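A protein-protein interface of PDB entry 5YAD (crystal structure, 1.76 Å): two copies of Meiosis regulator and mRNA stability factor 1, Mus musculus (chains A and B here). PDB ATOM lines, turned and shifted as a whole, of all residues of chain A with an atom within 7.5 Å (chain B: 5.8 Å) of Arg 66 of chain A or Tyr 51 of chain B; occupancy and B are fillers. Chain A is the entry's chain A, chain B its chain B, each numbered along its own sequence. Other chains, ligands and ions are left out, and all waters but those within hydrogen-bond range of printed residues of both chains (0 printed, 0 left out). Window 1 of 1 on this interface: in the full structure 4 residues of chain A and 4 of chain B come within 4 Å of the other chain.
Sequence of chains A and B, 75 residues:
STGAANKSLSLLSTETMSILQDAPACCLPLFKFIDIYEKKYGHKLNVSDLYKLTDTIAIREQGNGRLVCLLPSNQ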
ATOM      1  N   LEU A  28       0.808  -4.752  23.872  1.00  0.00           N
ATOM      2  CA  LEU A  28       1.918  -4.887  24.827  1.00  0.00           C
ATOM      3  C   LEU A  28       1.681  -3.853  25.949  1.00  0.00           C
ATOM      4  O   LEU A  28       1.131  -2.789  25.685  1.00  0.00           O
ATOM      5  CB  LEU A  28       3.290  -4.604  24.223  1.00  0.00           C
ATOM      6  CG  LEU A  28       3.887  -5.645  23.320  1.00  0.00           C
ATOM      7  CD1 LEU A  28       5.260  -5.208  22.746  1.00  0.00           C
ATOM      8  CD2 LEU A  28       4.050  -7.003  24.087  1.00  0.00           C
ATOM      9  N   PRO A  29       2.061  -4.195  27.172  1.00  0.00           N
ATOM     10  CA  PRO A  29       2.101  -3.129  28.188  1.00  0.00           C
ATOM     11  C   PRO A  29       3.031  -2.043  27.747  1.00  0.00           C
ATOM     12  O   PRO A  29       4.073  -2.292  27.102  1.00  0.00           O
ATOM     13  CB  PRO A  29       2.726  -3.845  29.417  1.00  0.00           C
ATOM     14  CG  PRO A  29       2.891  -5.304  29.078  1.00  0.00           C
ATOM     15  CD  PRO A  29       2.752  -5.466  27.575  1.00  0.00           C
ATOM     16  N   LEU A  30       2.690  -0.786  28.116  1.00  0.00           N
ATOM     17  CA  LEU A  30       3.526   0.307  27.723  1.00  0.00           C
ATOM     18  C   LEU A  30       4.995   0.201  28.140  1.00  0.00           C
ATOM     19  O   LEU A  30       5.916   0.399  27.326  1.00  0.00           O
ATOM     20  CB  LEU A  30       2.892   1.638  28.179  1.00  0.00           C
ATOM     21  CG  LEU A  30       3.709   2.888  27.835  1.00  0.00           C
ATOM     22  CD1 LEU A  30       3.878   3.108  26.313  1.00  0.00           C
ATOM     23  CD2 LEU A  30       3.124   4.121  28.483  1.00  0.00           C
ATOM     24  N   PHE A  31       5.254  -0.252  29.375  1.00  0.00           N
ATOM     25  CA  PHE A  31       6.644  -0.318  29.844  1.00  0.00           C
ATOM     26  C   PHE A  31       7.471  -1.256  28.939  1.00  0.00           C
ATOM     27  O   PHE A  31       8.671  -1.032  28.682  1.00  0.00           O
ATOM     28  CB  PHE A  31       6.714  -0.721  31.379  1.00  0.00           C
ATOM     29  CG  PHE A  31       6.595  -2.214  31.617  1.00  0.00           C
ATOM     30  CD1 PHE A  31       5.371  -2.822  31.777  1.00  0.00           C
ATOM     31  CD2 PHE A  31       7.739  -2.999  31.602  1.00  0.00           C
ATOM     32  CE1 PHE A  31       5.242  -4.223  31.949  1.00  0.00           C
ATOM     33  CE2 PHE A  31       7.625  -4.390  31.791  1.00  0.00           C
ATOM     34  CZ  PHE A  31       6.409  -4.996  31.955  1.00  0.00           C
ATOM     35  N   LYS A  32       6.818  -2.300  28.492  1.00  0.00           N
ATOM     36  CA  LYS A  32       7.448  -3.355  27.688  1.00  0.00           C
ATOM     37  C   LYS A  32       7.646  -2.875  26.267  1.00  0.00           C
ATOM     38  O   LYS A  32       8.708  -3.063  25.660  1.00  0.00           O
ATOM     39  CB  LYS A  32       6.627  -4.628  27.717  1.00  0.00           C
ATOM     40  CG  LYS A  32       7.355  -5.786  27.107  1.00  0.00           C
ATOM     41  CD  LYS A  32       6.823  -7.059  27.713  1.00  0.00           C
ATOM     42  CE  LYS A  32       7.081  -8.297  26.847  1.00  0.00           C
ATOM     43  NZ  LYS A  32       6.330  -9.406  27.544  1.00  0.00           N
ATOM     44  N   ILE A  34       8.095   0.263  25.380  1.00  0.00           N
ATOM     45  CA  ILE A  34       9.212   1.196  25.488  1.00  0.00           C
ATOM     46  C   ILE A  34      10.576   0.466  25.474  1.00  0.00           C
ATOM     47  O   ILE A  34      11.460   0.789  24.729  1.00  0.00           O
ATOM     48  CB  ILE A  34       9.089   2.095  26.715  1.00  0.00           C
ATOM     49  CG1 ILE A  34       7.843   2.996  26.632  1.00  0.00           C
ATOM     50  CG2 ILE A  34      10.365   2.920  26.952  1.00  0.00           C
ATOM     51  CD1 ILE A  34       7.559   3.655  28.008  1.00  0.00           C
ATOM     52  N   VAL A  47       7.193   9.130  24.405  1.00  0.00           N
ATOM     53  CA  VAL A  47       5.888   8.499  24.555  1.00  0.00           C
ATOM     54  C   VAL A  47       4.755   9.334  24.058  1.00  0.00           C
ATOM     55  O   VAL A  47       3.743   8.818  23.523  1.00  0.00           O
ATOM     56  CB  VAL A  47       5.680   7.943  26.000  1.00  0.00           C
ATOM     57  CG1 VAL A  47       4.265   7.553  26.224  1.00  0.00           C
ATOM     58  CG2 VAL A  47       6.655   6.822  26.199  1.00  0.00           C
ATOM     59  N   SER A  48       4.839  10.655  24.241  1.00  0.00           N
ATOM     60  CA  SER A  48       3.816  11.517  23.659  1.00  0.00           C
ATOM     61  C   SER A  48       3.619  11.395  22.128  1.00  0.00           C
ATOM     62  O   SER A  48       2.520  11.650  21.639  1.00  0.00           O
ATOM     63  CB  SER A  48       4.037  12.984  24.034  1.00  0.00           C
ATOM     64  OG  SER A  48       5.258  13.460  23.528  1.00  0.00           O
ATOM     65  N   LEU A  50       3.442   8.570  20.616  1.00  0.00           N
ATOM     66  CA  LEU A  50       2.494   7.459  20.415  1.00  0.00           C
ATOM     67  C   LEU A  50       1.081   7.965  20.397  1.00  0.00           C
ATOM     68  O   LEU A  50       0.250   7.434  19.707  1.00  0.00           O
ATOM     69  CB  LEU A  50       2.679   6.364  21.537  1.00  0.00           C
ATOM     70  CG  LEU A  50       4.047   5.735  21.626  1.00  0.00           C
ATOM     71  CD1 LEU A  50       3.951   4.748  22.742  1.00  0.00           C
ATOM     72  CD2 LEU A  50       4.415   5.013  20.324  1.00  0.00           C
ATOM     73  N   TYR A  51       0.745   9.005  21.175  1.00  0.00           N
ATOM     74  CA  TYR A  51      -0.566   9.531  21.165  1.00  0.00           C
ATOM     75  C   TYR A  51      -0.919  10.336  19.882  1.00  0.00           C
ATOM     76  O   TYR A  51      -2.106  10.622  19.630  1.00  0.00           O
ATOM     77  CB  TYR A  51      -0.750  10.448  22.404  1.00  0.00           C
ATOM     78  CG  TYR A  51      -0.934   9.660  23.655  1.00  0.00           C
ATOM     79  CD1 TYR A  51      -2.189   9.160  24.004  1.00  0.00           C
ATOM     80  CD2 TYR A  51       0.140   9.315  24.420  1.00  0.00           C
ATOM     81  CE1 TYR A  51      -2.389   8.412  25.184  1.00  0.00           C
ATOM     82  CE2 TYR A  51      -0.018   8.555  25.584  1.00  0.00           C
ATOM     83  CZ  TYR A  51      -1.290   8.105  25.982  1.00  0.00           C
ATOM     84  OH  TYR A  51      -1.407   7.317  27.128  1.00  0.00           O
ATOM     85  N   ILE A  59      -4.105   3.523  22.930  1.00  0.00           N
ATOM     86  CA  ILE A  59      -3.403   3.286  24.188  1.00  0.00           C
ATOM     87  C   ILE A  59      -4.497   3.273  25.215  1.00  0.00           C
ATOM     88  O   ILE A  59      -5.224   4.235  25.342  1.00  0.00           O
ATOM     89  CB  ILE A  59      -2.377   4.352  24.449  1.00  0.00           C
ATOM     90  CG1 ILE A  59      -1.367   4.392  23.346  1.00  0.00           C
ATOM     91  CG2 ILE A  59      -1.666   4.111  25.798  1.00  0.00           C
ATOM     92  CD1 ILE A  59      -0.403   5.478  23.398  1.00  0.00           C
ATOM     93  N   ARG A  60      -4.682   2.170  25.890  1.00  0.00           N
ATOM     94  CA  ARG A  60      -5.773   1.980  26.829  1.00  0.00           C
ATOM     95  C   ARG A  60      -5.275   2.094  28.233  1.00  0.00           C
ATOM     96  O   ARG A  60      -4.188   1.577  28.598  1.00  0.00           O
ATOM     97  CB  ARG A  60      -6.387   0.606  26.623  1.00  0.00           C
ATOM     98  CG  ARG A  60      -7.003   0.461  25.237  1.00  0.00           C
ATOM     99  CD  ARG A  60      -7.813  -0.841  25.070  1.00  0.00           C
ATOM    100  NE  ARG A  60      -7.826  -1.207  23.640  1.00  0.00           N
ATOM    101  CZ  ARG A  60      -8.455  -0.535  22.657  1.00  0.00           C
ATOM    102  NH1 ARG A  60      -9.202   0.560  22.905  1.00  0.00           N
ATOM    103  NH2 ARG A  60      -8.352  -0.971  21.391  1.00  0.00           N
ATOM    104  N   GLU A  61      -6.042   2.811  29.064  1.00  0.00           N
ATOM    105  CA  GLU A  61      -5.744   2.877  30.446  1.00  0.00           C
ATOM    106  C   GLU A  61      -6.158   1.594  31.137  1.00  0.00           C
ATOM    107  O   GLU A  61      -7.249   1.113  30.936  1.00  0.00           O
ATOM    108  CB  GLU A  61      -6.466   4.046  31.115  1.00  0.00           C
ATOM    109  CG  GLU A  61      -6.055   5.369  30.445  1.00  0.00           C
ATOM    110  CD  GLU A  61      -4.680   5.950  30.938  1.00  0.00           C
ATOM    111  OE1 GLU A  61      -4.239   5.684  32.097  1.00  0.00           O
ATOM    112  OE2 GLU A  61      -4.065   6.651  30.113  1.00  0.00           O
ATOM    113  N   GLN A  62      -5.332   1.121  32.039  1.00  0.00           N
ATOM    114  CA  GLN A  62      -5.700   0.036  32.903  1.00  0.00           C
ATOM    115  C   GLN A  62      -5.292   0.398  34.288  1.00  0.00           C
ATOM    116  O   GLN A  62      -4.388   1.261  34.540  1.00  0.00           O
ATOM    117  CB  GLN A  62      -5.046  -1.304  32.460  1.00  0.00           C
ATOM    118  CG  GLN A  62      -5.546  -1.759  31.110  1.00  0.00           C
ATOM    119  CD  GLN A  62      -4.963  -3.118  30.708  1.00  0.00           C
ATOM    120  OE1 GLN A  62      -3.985  -3.574  31.299  1.00  0.00           O
ATOM    121  NE2 GLN A  62      -5.563  -3.751  29.739  1.00  0.00           N
ATOM    122  N   GLY A  63      -5.824  -0.350  35.232  1.00  0.00           N
ATOM    123  CA  GLY A  63      -5.508  -0.050  36.636  1.00  0.00           C
ATOM    124  C   GLY A  63      -4.054  -0.054  37.011  1.00  0.00           C
ATOM    125  O   GLY A  63      -3.649   0.801  37.783  1.00  0.00           O
ATOM    126  N   ASN A  64      -3.233  -0.980  36.440  1.00  0.00           N
ATOM    127  CA  ASN A  64      -1.854  -1.059  36.753  1.00  0.00           C
ATOM    128  C   ASN A  64      -0.909  -0.564  35.701  1.00  0.00           C
ATOM    129  O   ASN A  64       0.315  -0.709  35.813  1.00  0.00           O
ATOM    130  CB  ASN A  64      -1.533  -2.517  37.109  1.00  0.00           C
ATOM    131  CG  ASN A  64      -2.259  -2.968  38.338  1.00  0.00           C
ATOM    132  OD1 ASN A  64      -2.255  -2.229  39.325  1.00  0.00           O
ATOM    133  ND2 ASN A  64      -2.875  -4.179  38.312  1.00  0.00           N
ATOM    134  N   GLY A  65      -1.463   0.074  34.656  1.00  0.00           N
ATOM    135  CA  GLY A  65      -0.575   0.570  33.589  1.00  0.00           C
ATOM    136  C   GLY A  65      -1.288   0.533  32.236  1.00  0.00           C
ATOM    137  O   GLY A  65      -2.311  -0.091  32.030  1.00  0.00           O
ATOM    138  N   ARG A  66      -0.744   1.257  31.300  1.00  0.00           N
ATOM    139  CA  ARG A  66      -1.294   1.367  29.958  1.00  0.00           C
ATOM    140  C   ARG A  66      -0.939   0.139  29.092  1.00  0.00           C
ATOM    141  O   ARG A  66       0.130  -0.422  29.240  1.00  0.00           O
ATOM    142  CB  ARG A  66      -0.838   2.647  29.298  1.00  0.00           C
ATOM    143  CG  ARG A  66      -1.613   3.893  29.817  1.00  0.00           C
ATOM    144  CD  ARG A  66      -0.878   5.174  29.427  1.00  0.00           C
ATOM    145  NE  ARG A  66       0.326   5.437  30.177  1.00  0.00           N
ATOM    146  CZ  ARG A  66       1.132   6.465  29.968  1.00  0.00           C
ATOM    147  NH1 ARG A  66       0.927   7.282  28.960  1.00  0.00           N
ATOM    148  NH2 ARG A  66       2.203   6.637  30.718  1.00  0.00           N
ATOM    149  N   LEU A  67      -1.828  -0.064  28.107  1.00  0.00           N
ATOM    150  CA  LEU A  67      -1.686  -1.118  27.103  1.00  0.00           C
ATOM    151  C   LEU A  67      -1.685  -0.439  25.759  1.00  0.00           C
ATOM    152  O   LEU A  67      -2.618   0.276  25.454  1.00  0.00           O
ATOM    153  CB  LEU A  67      -2.961  -1.995  27.257  1.00  0.00           C
ATOM    154  CG  LEU A  67      -2.961  -3.321  26.486  1.00  0.00           C
ATOM    155  CD1 LEU A  67      -1.964  -4.330  27.083  1.00  0.00           C
ATOM    156  CD2 LEU A  67      -4.366  -3.926  26.378  1.00  0.00           C
ATOM    157  N   VAL A  68      -0.711  -0.770  24.920  1.00  0.00           N
ATOM    158  CA  VAL A  68      -0.546  -0.215  23.581  1.00  0.00           C
ATOM    159  C   VAL A  68      -1.094  -1.308  22.684  1.00  0.00           C
ATOM    160  O   VAL A  68      -0.534  -2.437  22.641  1.00  0.00           O
ATOM    161  CB  VAL A  68       0.951   0.058  23.264  1.00  0.00           C
ATOM    162  CG1 VAL A  68       1.093   0.689  21.901  1.00  0.00           C
ATOM    163  CG2 VAL A  68       1.574   0.944  24.332  1.00  0.00           C
ATOM    164  N   CYS A  69      -2.115  -0.938  21.884  1.00  0.00           N
ATOM    165  CA  CYS A  69      -2.894  -1.912  21.073  1.00  0.00           C
ATOM    166  C   CYS A  69      -2.884  -1.498  19.591  1.00  0.00           C
ATOM    167  O   CYS A  69      -3.284  -0.401  19.233  1.00  0.00           O
ATOM    168  CB  CYS A  69      -4.341  -1.964  21.486  1.00  0.00           C
ATOM    169  SG  CYS A  69      -4.512  -2.303  23.288  1.00  0.00           S
ATOM    170  N   VAL B  47      -9.965   8.967  31.314  1.00  0.00           N
ATOM    171  CA  VAL B  47      -8.594   9.568  31.104  1.00  0.00           C
ATOM    172  C   VAL B  47      -8.278   9.683  29.630  1.00  0.00           C
ATOM    173  O   VAL B  47      -7.708  10.681  29.140  1.00  0.00           O
ATOM    174  CB  VAL B  47      -7.541   8.828  31.944  1.00  0.00           C
ATOM    175  CG1 VAL B  47      -6.101   9.189  31.544  1.00  0.00           C
ATOM    176  CG2 VAL B  47      -7.776   9.042  33.430  1.00  0.00           C
ATOM    177  N   SER B  48      -8.675   8.696  28.832  1.00  0.00           N
ATOM    178  CA  SER B  48      -8.549   8.866  27.358  1.00  0.00           C
ATOM    179  C   SER B  48      -9.207  10.079  26.722  1.00  0.00           C
ATOM    180  O   SER B  48      -8.690  10.575  25.721  1.00  0.00           O
ATOM    181  CB  SER B  48      -8.945   7.621  26.605  1.00  0.00           C
ATOM    182  OG  SER B  48     -10.323   7.358  26.832  1.00  0.00           O
ATOM    183  N   ASP B  49     -10.351  10.539  27.222  1.00  0.00           N
ATOM    184  CA  ASP B  49     -10.940  11.791  26.763  1.00  0.00           C
ATOM    185  C   ASP B  49     -10.047  13.012  27.069  1.00  0.00           C
ATOM    186  O   ASP B  49      -9.995  13.954  26.266  1.00  0.00           O
ATOM    187  CB  ASP B  49     -12.324  12.060  27.358  1.00  0.00           C
ATOM    188  CG  ASP B  49     -13.455  11.316  26.642  1.00  0.00           C
ATOM    189  OD1 ASP B  49     -13.296  10.868  25.485  1.00  0.00           O
ATOM    190  OD2 ASP B  49     -14.512  11.212  27.283  1.00  0.00           O
ATOM    191  N   LEU B  50      -9.243  12.985  28.142  1.00  0.00           N
ATOM    192  CA  LEU B  50      -8.360  14.085  28.410  1.00  0.00           C
ATOM    193  C   LEU B  50      -7.366  14.287  27.274  1.00  0.00           C
ATOM    194  O   LEU B  50      -6.944  15.377  26.959  1.00  0.00           O
ATOM    195  CB  LEU B  50      -7.482  13.798  29.660  1.00  0.00           C
ATOM    196  CG  LEU B  50      -7.998  14.035  31.021  1.00  0.00           C
ATOM    197  CD1 LEU B  50      -6.896  13.737  32.064  1.00  0.00           C
ATOM    198  CD2 LEU B  50      -8.491  15.459  31.219  1.00  0.00           C
ATOM    199  N   TYR B  51      -6.949  13.193  26.673  1.00  0.00           N
ATOM    200  CA  TYR B  51      -6.000  13.243  25.553  1.00  0.00           C
ATOM    201  C   TYR B  51      -6.595  13.866  24.292  1.00  0.00           C
ATOM    202  O   TYR B  51      -5.841  14.296  23.427  1.00  0.00           O
ATOM    203  CB  TYR B  51      -5.476  11.830  25.223  1.00  0.00           C
ATOM    204  CG  TYR B  51      -4.373  11.398  26.168  1.00  0.00           C
ATOM    205  CD1 TYR B  51      -3.065  11.791  25.919  1.00  0.00           C
ATOM    206  CD2 TYR B  51      -4.617  10.579  27.280  1.00  0.00           C
ATOM    207  CE1 TYR B  51      -1.995  11.439  26.792  1.00  0.00           C
ATOM    208  CE2 TYR B  51      -3.562  10.249  28.124  1.00  0.00           C
ATOM    209  CZ  TYR B  51      -2.281  10.704  27.857  1.00  0.00           C
ATOM    210  OH  TYR B  51      -1.241  10.330  28.659  1.00  0.00           O
ATOM    211  N   LYS B  52      -7.917  13.931  24.231  1.00  0.00           N
ATOM    212  CA  LYS B  52      -8.579  14.705  23.173  1.00  0.00           C
ATOM    213  C   LYS B  52      -8.652  16.210  23.384  1.00  0.00           C
ATOM    214  O   LYS B  52      -8.977  16.955  22.442  1.00  0.00           O
ATOM    215  CB  LYS B  52      -9.957  14.138  22.924  1.00  0.00           C
ATOM    216  CG  LYS B  52      -9.855  12.756  22.355  1.00  0.00           C
ATOM    217  CD  LYS B  52     -11.195  12.078  22.343  1.00  0.00           C
ATOM    218  CE  LYS B  52     -11.012  10.776  21.594  1.00  0.00           C
ATOM    219  NZ  LYS B  52     -12.338  10.231  21.250  1.00  0.00           N
ATOM    220  N   LEU B  53      -8.302  16.698  24.568  1.00  0.00           N
ATOM    221  CA  LEU B  53      -8.326  18.139  24.864  1.00  0.00           C
ATOM    222  C   LEU B  53      -7.054  18.857  24.496  1.00  0.00           C
ATOM    223  O   LEU B  53      -6.502  19.638  25.268  1.00  0.00           O
ATOM    224  CB  LEU B  53      -8.712  18.349  26.332  1.00  0.00           C
ATOM    225  CG  LEU B  53      -9.941  17.587  26.849  1.00  0.00           C
ATOM    226  CD1 LEU B  53     -10.142  17.947  28.309  1.00  0.00           C
ATOM    227  CD2 LEU B  53     -11.140  18.002  25.986  1.00  0.00           C
ATOM    228  N   THR B  54      -6.643  18.707  23.227  1.00  0.00           N
ATOM    229  CA  THR B  54      -5.357  19.205  22.786  1.00  0.00           C
ATOM    230  C   THR B  54      -5.304  20.727  22.682  1.00  0.00           C
ATOM    231  O   THR B  54      -4.226  21.238  22.698  1.00  0.00           O
ATOM    232  CB  THR B  54      -4.930  18.548  21.440  1.00  0.00           C
ATOM    233  OG1 THR B  54      -6.023  18.654  20.553  1.00  0.00           O
ATOM    234  CG2 THR B  54      -4.657  17.089  21.606  1.00  0.00           C
ATOM    235  N   ILE B  57      -5.240  21.326  27.432  1.00  0.00           N
ATOM    236  CA  ILE B  57      -4.163  20.780  28.286  1.00  0.00           C
ATOM    237  C   ILE B  57      -3.087  20.038  27.524  1.00  0.00           C
ATOM    238  O   ILE B  57      -3.301  19.610  26.361  1.00  0.00           O
ATOM    239  CB  ILE B  57      -4.710  19.775  29.347  1.00  0.00           C
ATOM    240  CG1 ILE B  57      -5.561  18.707  28.650  1.00  0.00           C
ATOM    241  CG2 ILE B  57      -5.480  20.518  30.406  1.00  0.00           C
ATOM    242  CD1 ILE B  57      -5.710  17.484  29.497  1.00  0.00           C
ATOM    243  N   ILE B  59      -0.613  16.667  28.398  1.00  0.00           N
ATOM    244  CA  ILE B  59      -0.296  15.646  29.378  1.00  0.00           C
ATOM    245  C   ILE B  59       1.189  15.340  29.178  1.00  0.00           C
ATOM    246  O   ILE B  59       1.608  14.952  28.066  1.00  0.00           O
ATOM    247  CB  ILE B  59      -1.189  14.462  29.208  1.00  0.00           C
ATOM    248  CG1 ILE B  59      -2.634  14.889  29.462  1.00  0.00           C
ATOM    249  CG2 ILE B  59      -0.807  13.371  30.203  1.00  0.00           C
ATOM    250  CD1 ILE B  59      -3.674  13.886  29.155  1.00  0.00           C
ATOM    251  N   GLU B  61       4.656  13.381  29.876  1.00  0.00           N
ATOM    252  CA  GLU B  61       5.209  12.116  30.372  1.00  0.00           C
ATOM    253  C   GLU B  61       6.415  12.494  31.161  1.00  0.00           C
ATOM    254  O   GLU B  61       7.279  13.309  30.733  1.00  0.00           O
ATOM    255  CB  GLU B  61       5.668  11.254  29.218  1.00  0.00           C
ATOM    256  CG  GLU B  61       4.549  10.817  28.429  1.00  0.00           C
ATOM    257  CD  GLU B  61       3.804   9.559  29.085  1.00  0.00           C
ATOM    258  OE1 GLU B  61       4.296   8.681  29.960  1.00  0.00           O
ATOM    259  OE2 GLU B  61       2.621   9.577  28.717  1.00  0.00           O
ATOM    260  N   ARG B  66       2.671  10.957  35.037  1.00  0.00           N
ATOM    261  CA  ARG B  66       2.169  11.997  34.133  1.00  0.00           C
ATOM    262  C   ARG B  66       1.779  13.227  34.864  1.00  0.00           C
ATOM    263  O   ARG B  66       1.275  13.147  35.993  1.00  0.00           O
ATOM    264  CB  ARG B  66       1.030  11.473  33.262  1.00  0.00           C
ATOM    265  CG  ARG B  66       1.526  10.508  32.143  1.00  0.00           C
ATOM    266  CD  ARG B  66       0.373   9.857  31.433  1.00  0.00           C
ATOM    267  NE  ARG B  66      -0.158   8.767  32.231  1.00  0.00           N
ATOM    268  CZ  ARG B  66      -1.284   8.074  31.884  1.00  0.00           C
ATOM    269  NH1 ARG B  66      -1.984   8.374  30.807  1.00  0.00           N
ATOM    270  NH2 ARG B  66      -1.701   7.099  32.643  1.00  0.00           N
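OH of Tyr 51 of chain B is in hydrogen-bond range of NH1 of Arg 66 of chain B (3.0 Å). N of Leu 30 of chain A sits at hydrogen-bond distance from O of Arg 66 of chain A, at 2.8 Å. OH of Tyr 51 of chain A lies within hydrogen-bond range of NH1 of Arg 66 of chain A (3.0 Å).
Val 47 of chain A touches Glu 61 of chain B, and with the chains exchanged Glu 61 of chain A touches Val 47 of chain B. Tyr 51 of chain A touches its own counterpart, Tyr 51 of chain B. Tyr 51 of chain A touches Arg 66 of chain B, and with the chains exchanged Arg 66 of chain A touches Tyr 51 of chain B. Glu 61 of chain A touches Arg 66 of chain B, and with the chains exchanged Arg 66 of chain A touches Glu 61 of chain B. 7 positions are printed for both chains. Of the 8 pairs that touch across the chains among the printed residues, 8 have their exchanged pair printed and touching as well.
Among the printed residues, pairs that only touch across the chains: Arg 66 of chain A with Arg 66 of chain B, Val 47 of chain A with Glu 61 of chain B, Glu 61 of chain A with Val 47 of chain B, Arg 66 of chain A with Tyr 51 of chain B and Tyr 51 of chain A with Arg 66 of chain B.
Arg 66 of chain A touches three residues of chain B. Tyr 51 of chain B touches just these residues of chain A: Tyr 51 and Arg 66. Of the printed residues of chain B, Val 47 of chain A touches Glu 61 (3.5 Å). Printed residues of chain B within 4 Å of Glu 61 of chain A: Val 47 (3.6 Å) and Arg 66 (2.8 Å). Of the printed residues of chain B, Tyr 51 of chain A touches Tyr 51 and Arg 66. Of the printed residues of chain A, Val 47 of chain B touches Glu 61. Leu 30 of chain A touches none of the printed residues of chain B. Leu 50 of chain B touches none of the printed residues of chain A. The nearest printed residue of chain B that does not touch Arg 66 of chain A is Ile 59 of chain B (6.5 Å). The nearest residue of chain A that does not touch Tyr 51 of chain B is Glu 61 of chain A (4.1 Å). The nearest printed residue of chain A that does not touch Glu 61 of chain B is Ser 48 of chain A (4.2 Å).
OE2 of Glu 61 of chain A is in salt-bridge range of NH1 of Arg 66 of chain B (2.8 Å). The side-chain hydroxyl (OH) of Tyr 51 of chain A sits at hydrogen-bond distance from the side-chain hydroxyl (OH) of Tyr 51 of chain B, 3.4 Å away. NH1 of Arg 66 of chain A lies within salt-bridge range of OE2 of Glu 61 of chain B.
Of the 21 printed residues of chain A, 4 touch a printed residue of chain B. Printed residues of chain A that touch a printed residue of chain B: Val 47, Tyr 51, Glu 61 and Arg 66. Of the 12 printed residues of chain B, 4 touch a printed residue of chain A. Printed residues of chain B that touch a printed residue of chain A: Val 47, Tyr 51, Glu 61 and Arg 66. Hydrophobic or aromatic side chains of chain B within 4 Å of the printed part of chain A: Val 47 and Tyr 51. Along chain B the printed residues that touch a printed residue of chain A span positions 47 to 66.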
